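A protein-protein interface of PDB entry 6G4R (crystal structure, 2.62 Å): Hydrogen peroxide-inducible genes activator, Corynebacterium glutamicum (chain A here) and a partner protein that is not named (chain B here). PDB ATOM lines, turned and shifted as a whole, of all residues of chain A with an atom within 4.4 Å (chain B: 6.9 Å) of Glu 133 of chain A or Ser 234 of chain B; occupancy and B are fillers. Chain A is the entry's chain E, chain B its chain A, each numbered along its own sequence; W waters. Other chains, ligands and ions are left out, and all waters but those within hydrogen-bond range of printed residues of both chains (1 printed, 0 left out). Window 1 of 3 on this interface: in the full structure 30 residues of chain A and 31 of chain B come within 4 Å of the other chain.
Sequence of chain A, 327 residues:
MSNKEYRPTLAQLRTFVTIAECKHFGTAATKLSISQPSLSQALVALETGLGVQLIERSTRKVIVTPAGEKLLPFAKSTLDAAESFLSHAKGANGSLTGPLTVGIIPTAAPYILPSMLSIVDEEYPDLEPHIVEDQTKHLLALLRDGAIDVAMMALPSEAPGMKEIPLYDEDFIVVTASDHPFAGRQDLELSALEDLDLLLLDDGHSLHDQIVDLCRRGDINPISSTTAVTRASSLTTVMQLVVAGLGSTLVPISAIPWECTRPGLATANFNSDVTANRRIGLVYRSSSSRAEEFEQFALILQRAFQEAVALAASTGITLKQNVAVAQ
N of Glu 133 of chain A lies within hydrogen-bond range of O of Arg 231 of chain B (2.9 Å). The guanidinium group (NH2) of Arg 231 of chain B is in salt-bridge range of the side-chain carboxylate (OD2) of Asp 134 of chain A, 2.9 Å away. The backbone carbonyl oxygen of Ile 131 of chain A sits at hydrogen-bond distance from the backbone NH of Arg 231 of chain B. OG1 of Thr 237 of chain B sits at hydrogen-bond distance from OE2 of Glu 133 of chain A, 2.5 Å away. The backbone NH of Ser 233 of chain B sits at hydrogen-bond distance from the side-chain carboxylate of Glu 133 of chain A, 2.6 Å away. OG1 of Thr 230 of chain B lies within hydrogen-bond range of N of Ile 131 of chain A, 3.4 Å away. OE1 of Glu 133 of chain A lies within hydrogen-bond range of N of Ser 234 of chain B (3.2 Å).
O of Ile 104 of chain A lies within hydrogen-bond range of N of Asp 134 of chain A, at 3.4 Å. The side-chain hydroxyl (OG) of Ser 234 of chain B sits at hydrogen-bond distance from the side-chain hydroxyl (OG1) of Thr 237 of chain B. The backbone NH of Ile 104 of chain A lies within hydrogen-bond range of the backbone carbonyl oxygen of Val 132 of chain A (2.9 Å).
Among the printed residues, merely in contact across the chains: Pro 110 of chain A with Thr 237 of chain B, Glu 133 of chain A with Ala 232 of chain B, Val 132 of chain A with Arg 231 of chain B, Pro 110 of chain A with Thr 236 of chain B and Val 132 of chain A with Val 229 of chain B.
Water W1 lies within hydrogen-bond range of the side-chain carboxylate (OE2) of Glu 133 of chain A (2.6 Å), the side-chain hydroxyl (OG) of Ser 234 of chain B (2.8 Å), the backbone carbonyl oxygen (O) of Pro 106 of chain A (2.9 Å) and the side-chain hydroxyl (OG1) of Thr 237 of chain B (3.5 Å).
Glu 133 of chain A touches just these residues of chain B: Arg 231 (2.9 Å), Ala 232 (3.4 Å), Ser 233 (2.6 Å), Ser 234 (3.2 Å) and Thr 237 (2.5 Å). Of chain A, only Glu 133 comes within 4 Å of Ser 234 of chain B. Of the printed residues of chain A, Ser 233 of chain B touches Glu 133. Of the printed residues of chain B, Pro 110 of chain A touches Thr 236 and Thr 237. Printed residues of chain A within 4 Å of Val 229 of chain B: Val 132. Printed residues of chain B within 4 Å of Ile 131 of chain A: Thr 230 and Arg 231. Printed residues of chain A within 4 Å of Ala 232 of chain B: Glu 133. Leu 201 of chain B touches none of the printed residues of chain A. The nearest printed residue of chain A that does not touch Thr 237 of chain B is Ala 109 of chain A (4.1 Å).
Of the 8 printed residues of chain A, 5 touch a printed residue of chain B. Hydrophobic or aromatic side chains of chain A that line the printed part of chain B: Pro 110 and Val 132. Hydrophobic or aromatic side chains of chain B within 4 Å of the printed part of chain A: Ala 232.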
ATOM      1  N   ILE A 104      12.794  -5.958 -22.853  1.00  0.00           N
ATOM      2  CA  ILE A 104      12.574  -6.145 -21.425  1.00  0.00           C
ATOM      3  C   ILE A 104      13.751  -6.912 -20.837  1.00  0.00           C
ATOM      4  O   ILE A 104      14.237  -7.879 -21.436  1.00  0.00           O
ATOM      5  CB  ILE A 104      11.249  -6.885 -21.141  1.00  0.00           C
ATOM      6  CG1 ILE A 104      10.100  -6.266 -21.943  1.00  0.00           C
ATOM      7  CG2 ILE A 104      10.923  -6.838 -19.660  1.00  0.00           C
ATOM      8  CD1 ILE A 104       8.784  -6.999 -21.797  1.00  0.00           C
ATOM      9  N   PRO A 106      15.740  -9.489 -18.330  1.00  0.00           N
ATOM     10  CA  PRO A 106      15.301 -10.856 -18.000  1.00  0.00           C
ATOM     11  C   PRO A 106      14.754 -11.010 -16.591  1.00  0.00           C
ATOM     12  O   PRO A 106      13.981 -11.946 -16.351  1.00  0.00           O
ATOM     13  CB  PRO A 106      16.571 -11.697 -18.194  1.00  0.00           C
ATOM     14  CG  PRO A 106      17.530 -10.821 -18.941  1.00  0.00           C
ATOM     15  CD  PRO A 106      17.187  -9.416 -18.580  1.00  0.00           C
ATOM     16  N   ALA A 109      10.936  -9.717 -17.406  1.00  0.00           N
ATOM     17  CA  ALA A 109      10.129 -10.179 -18.536  1.00  0.00           C
ATOM     18  C   ALA A 109       9.146 -11.283 -18.164  1.00  0.00           C
ATOM     19  O   ALA A 109       7.931 -11.086 -18.339  1.00  0.00           O
ATOM     20  CB  ALA A 109      11.056 -10.593 -19.683  1.00  0.00           C
ATOM     21  N   PRO A 110       9.574 -12.446 -17.651  1.00  0.00           N
ATOM     22  CA  PRO A 110       8.617 -13.551 -17.468  1.00  0.00           C
ATOM     23  C   PRO A 110       7.578 -13.294 -16.390  1.00  0.00           C
ATOM     24  O   PRO A 110       6.618 -14.068 -16.287  1.00  0.00           O
ATOM     25  CB  PRO A 110       9.517 -14.733 -17.096  1.00  0.00           C
ATOM     26  CG  PRO A 110      10.653 -14.104 -16.390  1.00  0.00           C
ATOM     27  CD  PRO A 110      10.889 -12.778 -17.069  1.00  0.00           C
ATOM     28  N   ILE A 131       8.513  -8.737 -28.538  1.00  0.00           N
ATOM     29  CA  ILE A 131       9.208  -8.757 -27.256  1.00  0.00           C
ATOM     30  C   ILE A 131      10.635  -9.236 -27.472  1.00  0.00           C
ATOM     31  O   ILE A 131      10.861 -10.278 -28.098  1.00  0.00           O
ATOM     32  CB  ILE A 131       8.476  -9.649 -26.238  1.00  0.00           C
ATOM     33  CG1 ILE A 131       7.061  -9.121 -25.992  1.00  0.00           C
ATOM     34  CG2 ILE A 131       9.256  -9.726 -24.935  1.00  0.00           C
ATOM     35  CD1 ILE A 131       7.022  -7.698 -25.477  1.00  0.00           C
ATOM     36  N   VAL A 132      11.595  -8.480 -26.948  1.00  0.00           N
ATOM     37  CA  VAL A 132      13.012  -8.824 -27.012  1.00  0.00           C
ATOM     38  C   VAL A 132      13.535  -8.865 -25.583  1.00  0.00           C
ATOM     39  O   VAL A 132      13.589  -7.831 -24.906  1.00  0.00           O
ATOM     40  CB  VAL A 132      13.811  -7.830 -27.865  1.00  0.00           C
ATOM     41  CG1 VAL A 132      15.300  -8.115 -27.754  1.00  0.00           C
ATOM     42  CG2 VAL A 132      13.359  -7.893 -29.316  1.00  0.00           C
ATOM     43  N   GLU A 133      13.913 -10.052 -25.120  1.00  0.00           N
ATOM     44  CA  GLU A 133      14.435 -10.235 -23.772  1.00  0.00           C
ATOM     45  C   GLU A 133      15.949 -10.388 -23.832  1.00  0.00           C
ATOM     46  O   GLU A 133      16.455 -11.360 -24.403  1.00  0.00           O
ATOM     47  CB  GLU A 133      13.812 -11.454 -23.095  1.00  0.00           C
ATOM     48  CG  GLU A 133      14.295 -11.660 -21.667  1.00  0.00           C
ATOM     49  CD  GLU A 133      14.011 -13.054 -21.147  1.00  0.00           C
ATOM     50  OE1 GLU A 133      14.065 -14.008 -21.950  1.00  0.00           O
ATOM     51  OE2 GLU A 133      13.734 -13.194 -19.938  1.00  0.00           O
ATOM     52  N   ASP A 134      16.662  -9.434 -23.244  1.00  0.00           N
ATOM     53  CA  ASP A 134      18.114  -9.499 -23.147  1.00  0.00           C
ATOM     54  C   ASP A 134      18.555  -8.564 -22.028  1.00  0.00           C
ATOM     55  O   ASP A 134      17.742  -7.862 -21.422  1.00  0.00           O
ATOM     56  CB  ASP A 134      18.776  -9.147 -24.483  1.00  0.00           C
ATOM     57  CG  ASP A 134      19.970 -10.030 -24.789  1.00  0.00           C
ATOM     58  OD1 ASP A 134      20.845 -10.174 -23.910  1.00  0.00           O
ATOM     59  OD2 ASP A 134      20.030 -10.585 -25.907  1.00  0.00           O
ATOM     60  N   TYR B 111      17.603 -27.690 -13.936  1.00  0.00           N
ATOM     61  CA  TYR B 111      16.902 -28.964 -14.005  1.00  0.00           C
ATOM     62  C   TYR B 111      17.772 -30.142 -13.593  1.00  0.00           C
ATOM     63  O   TYR B 111      17.237 -31.217 -13.302  1.00  0.00           O
ATOM     64  CB  TYR B 111      16.364 -29.183 -15.424  1.00  0.00           C
ATOM     65  CG  TYR B 111      15.775 -27.923 -16.018  1.00  0.00           C
ATOM     66  CD1 TYR B 111      14.860 -27.159 -15.302  1.00  0.00           C
ATOM     67  CD2 TYR B 111      16.155 -27.479 -17.277  1.00  0.00           C
ATOM     68  CE1 TYR B 111      14.328 -26.000 -15.830  1.00  0.00           C
ATOM     69  CE2 TYR B 111      15.627 -26.317 -17.813  1.00  0.00           C
ATOM     70  CZ  TYR B 111      14.713 -25.584 -17.084  1.00  0.00           C
ATOM     71  OH  TYR B 111      14.181 -24.428 -17.604  1.00  0.00           O
ATOM     72  N   LEU B 201      15.598 -21.196 -28.157  1.00  0.00           N
ATOM     73  CA  LEU B 201      16.783 -20.913 -27.366  1.00  0.00           C
ATOM     74  C   LEU B 201      17.970 -21.699 -27.911  1.00  0.00           C
ATOM     75  O   LEU B 201      17.813 -22.670 -28.655  1.00  0.00           O
ATOM     76  CB  LEU B 201      16.551 -21.255 -25.894  1.00  0.00           C
ATOM     77  CG  LEU B 201      15.590 -20.339 -25.144  1.00  0.00           C
ATOM     78  CD1 LEU B 201      15.099 -21.024 -23.892  1.00  0.00           C
ATOM     79  CD2 LEU B 201      16.273 -19.034 -24.807  1.00  0.00           C
ATOM     80  N   VAL B 229      12.926  -9.192 -34.237  1.00  0.00           N
ATOM     81  CA  VAL B 229      11.815 -10.121 -34.092  1.00  0.00           C
ATOM     82  C   VAL B 229      11.767 -10.589 -32.643  1.00  0.00           C
ATOM     83  O   VAL B 229      12.723 -10.425 -31.881  1.00  0.00           O
ATOM     84  CB  VAL B 229      11.943 -11.310 -35.072  1.00  0.00           C
ATOM     85  CG1 VAL B 229      10.607 -12.019 -35.253  1.00  0.00           C
ATOM     86  CG2 VAL B 229      12.474 -10.833 -36.414  1.00  0.00           C
ATOM     87  N   THR B 230      10.635 -11.172 -32.252  1.00  0.00           N
ATOM     88  CA  THR B 230      10.476 -11.646 -30.884  1.00  0.00           C
ATOM     89  C   THR B 230      11.502 -12.726 -30.564  1.00  0.00           C
ATOM     90  O   THR B 230      11.681 -13.682 -31.326  1.00  0.00           O
ATOM     91  CB  THR B 230       9.058 -12.177 -30.671  1.00  0.00           C
ATOM     92  OG1 THR B 230       8.112 -11.133 -30.936  1.00  0.00           O
ATOM     93  CG2 THR B 230       8.877 -12.662 -29.241  1.00  0.00           C
ATOM     94  N   ARG B 231      12.173 -12.568 -29.423  1.00  0.00           N
ATOM     95  CA  ARG B 231      13.280 -13.432 -29.037  1.00  0.00           C
ATOM     96  C   ARG B 231      13.441 -13.364 -27.528  1.00  0.00           C
ATOM     97  O   ARG B 231      13.528 -12.267 -26.968  1.00  0.00           O
ATOM     98  CB  ARG B 231      14.597 -13.010 -29.686  1.00  0.00           C
ATOM     99  CG  ARG B 231      15.683 -14.062 -29.533  1.00  0.00           C
ATOM    100  CD  ARG B 231      16.999 -13.576 -30.082  1.00  0.00           C
ATOM    101  NE  ARG B 231      17.269 -12.242 -29.556  1.00  0.00           N
ATOM    102  CZ  ARG B 231      17.772 -12.014 -28.346  1.00  0.00           C
ATOM    103  NH1 ARG B 231      18.055 -13.032 -27.543  1.00  0.00           N
ATOM    104  NH2 ARG B 231      17.985 -10.771 -27.934  1.00  0.00           N
ATOM    105  N   ALA B 232      13.484 -14.520 -26.874  1.00  0.00           N
ATOM    106  CA  ALA B 232      13.675 -14.578 -25.434  1.00  0.00           C
ATOM    107  C   ALA B 232      14.985 -15.289 -25.118  1.00  0.00           C
ATOM    108  O   ALA B 232      15.531 -16.029 -25.941  1.00  0.00           O
ATOM    109  CB  ALA B 232      12.505 -15.287 -24.743  1.00  0.00           C
ATOM    110  N   SER B 233      15.489 -15.049 -23.906  1.00  0.00           N
ATOM    111  CA  SER B 233      16.758 -15.611 -23.464  1.00  0.00           C
ATOM    112  C   SER B 233      16.615 -16.712 -22.421  1.00  0.00           C
ATOM    113  O   SER B 233      17.616 -17.354 -22.086  1.00  0.00           O
ATOM    114  CB  SER B 233      17.660 -14.502 -22.902  1.00  0.00           C
ATOM    115  OG  SER B 233      17.185 -14.040 -21.650  1.00  0.00           O
ATOM    116  N   SER B 234      15.411 -16.952 -21.905  1.00  0.00           N
ATOM    117  CA  SER B 234      15.194 -17.959 -20.878  1.00  0.00           C
ATOM    118  C   SER B 234      13.938 -18.752 -21.203  1.00  0.00           C
ATOM    119  O   SER B 234      13.037 -18.262 -21.889  1.00  0.00           O
ATOM    120  CB  SER B 234      15.073 -17.327 -19.485  1.00  0.00           C
ATOM    121  OG  SER B 234      13.887 -16.560 -19.378  1.00  0.00           O
ATOM    122  N   LEU B 235      13.889 -19.991 -20.705  1.00  0.00           N
ATOM    123  CA  LEU B 235      12.725 -20.840 -20.946  1.00  0.00           C
ATOM    124  C   LEU B 235      11.475 -20.274 -20.286  1.00  0.00           C
ATOM    125  O   LEU B 235      10.379 -20.349 -20.853  1.00  0.00           O
ATOM    126  CB  LEU B 235      12.990 -22.261 -20.445  1.00  0.00           C
ATOM    127  CG  LEU B 235      13.649 -23.230 -21.426  1.00  0.00           C
ATOM    128  CD1 LEU B 235      13.917 -24.572 -20.769  1.00  0.00           C
ATOM    129  CD2 LEU B 235      12.758 -23.407 -22.640  1.00  0.00           C
ATOM    130  N   THR B 236      11.617 -19.707 -19.085  1.00  0.00           N
ATOM    131  CA  THR B 236      10.448 -19.175 -18.391  1.00  0.00           C
ATOM    132  C   THR B 236       9.818 -18.015 -19.151  1.00  0.00           C
ATOM    133  O   THR B 236       8.598 -17.828 -19.095  1.00  0.00           O
ATOM    134  CB  THR B 236      10.823 -18.751 -16.967  1.00  0.00           C
ATOM    135  OG1 THR B 236       9.662 -18.249 -16.293  1.00  0.00           O
ATOM    136  CG2 THR B 236      11.908 -17.681 -16.981  1.00  0.00           C
ATOM    137  N   THR B 237      10.623 -17.231 -19.872  1.00  0.00           N
ATOM    138  CA  THR B 237      10.072 -16.164 -20.701  1.00  0.00           C
ATOM    139  C   THR B 237       9.444 -16.717 -21.976  1.00  0.00           C
ATOM    140  O   THR B 237       8.384 -16.244 -22.403  1.00  0.00           O
ATOM    141  CB  THR B 237      11.158 -15.144 -21.038  1.00  0.00           C
ATOM    142  OG1 THR B 237      11.697 -14.601 -19.824  1.00  0.00           O
ATOM    143  CG2 THR B 237      10.586 -14.008 -21.876  1.00  0.00           C
ATOM    144  N   VAL B 238      10.084 -17.714 -22.592  1.00  0.00           N
ATOM    145  CA  VAL B 238       9.517 -18.345 -23.782  1.00  0.00           C
ATOM    146  C   VAL B 238       8.151 -18.942 -23.470  1.00  0.00           C
ATOM    147  O   VAL B 238       7.220 -18.852 -24.278  1.00  0.00           O
ATOM    148  CB  VAL B 238      10.485 -19.410 -24.335  1.00  0.00           C
ATOM    149  CG1 VAL B 238       9.817 -20.216 -25.436  1.00  0.00           C
ATOM    150  CG2 VAL B 238      11.757 -18.763 -24.849  1.00  0.00           C
ATOM    151  N   MET B 239       8.008 -19.546 -22.286  1.00  0.00           N
ATOM    152  CA  MET B 239       6.738 -20.162 -21.918  1.00  0.00           C
ATOM    153  C   MET B 239       5.615 -19.136 -21.863  1.00  0.00           C
ATOM    154  O   MET B 239       4.495 -19.407 -22.311  1.00  0.00           O
ATOM    155  CB  MET B 239       6.873 -20.884 -20.578  1.00  0.00           C
ATOM    156  CG  MET B 239       7.672 -22.165 -20.660  1.00  0.00           C
ATOM    157  SD  MET B 239       7.187 -23.155 -22.083  1.00  0.00           S
ATOM    158  CE  MET B 239       8.034 -24.686 -21.721  1.00  0.00           C
ATOM    159  N   GLU B 259       8.697 -26.067 -16.007  1.00  0.00           N
ATOM    160  CA  GLU B 259       8.262 -25.071 -16.980  1.00  0.00           C
ATOM    161  C   GLU B 259       6.981 -25.424 -17.722  1.00  0.00           C
ATOM    162  O   GLU B 259       6.357 -24.516 -18.285  1.00  0.00           O
ATOM    163  CB  GLU B 259       9.365 -24.818 -18.021  1.00  0.00           C
ATOM    164  CG  GLU B 259      10.751 -24.553 -17.443  1.00  0.00           C
ATOM    165  CD  GLU B 259      10.845 -23.227 -16.711  1.00  0.00           C
ATOM    166  OE1 GLU B 259      11.728 -23.092 -15.838  1.00  0.00           O
ATOM    167  OE2 GLU B 259      10.039 -22.321 -17.007  1.00  0.00           O
HETATM  168  O   HOH W   1      14.474 -14.393 -17.732  1.00  0.00           O
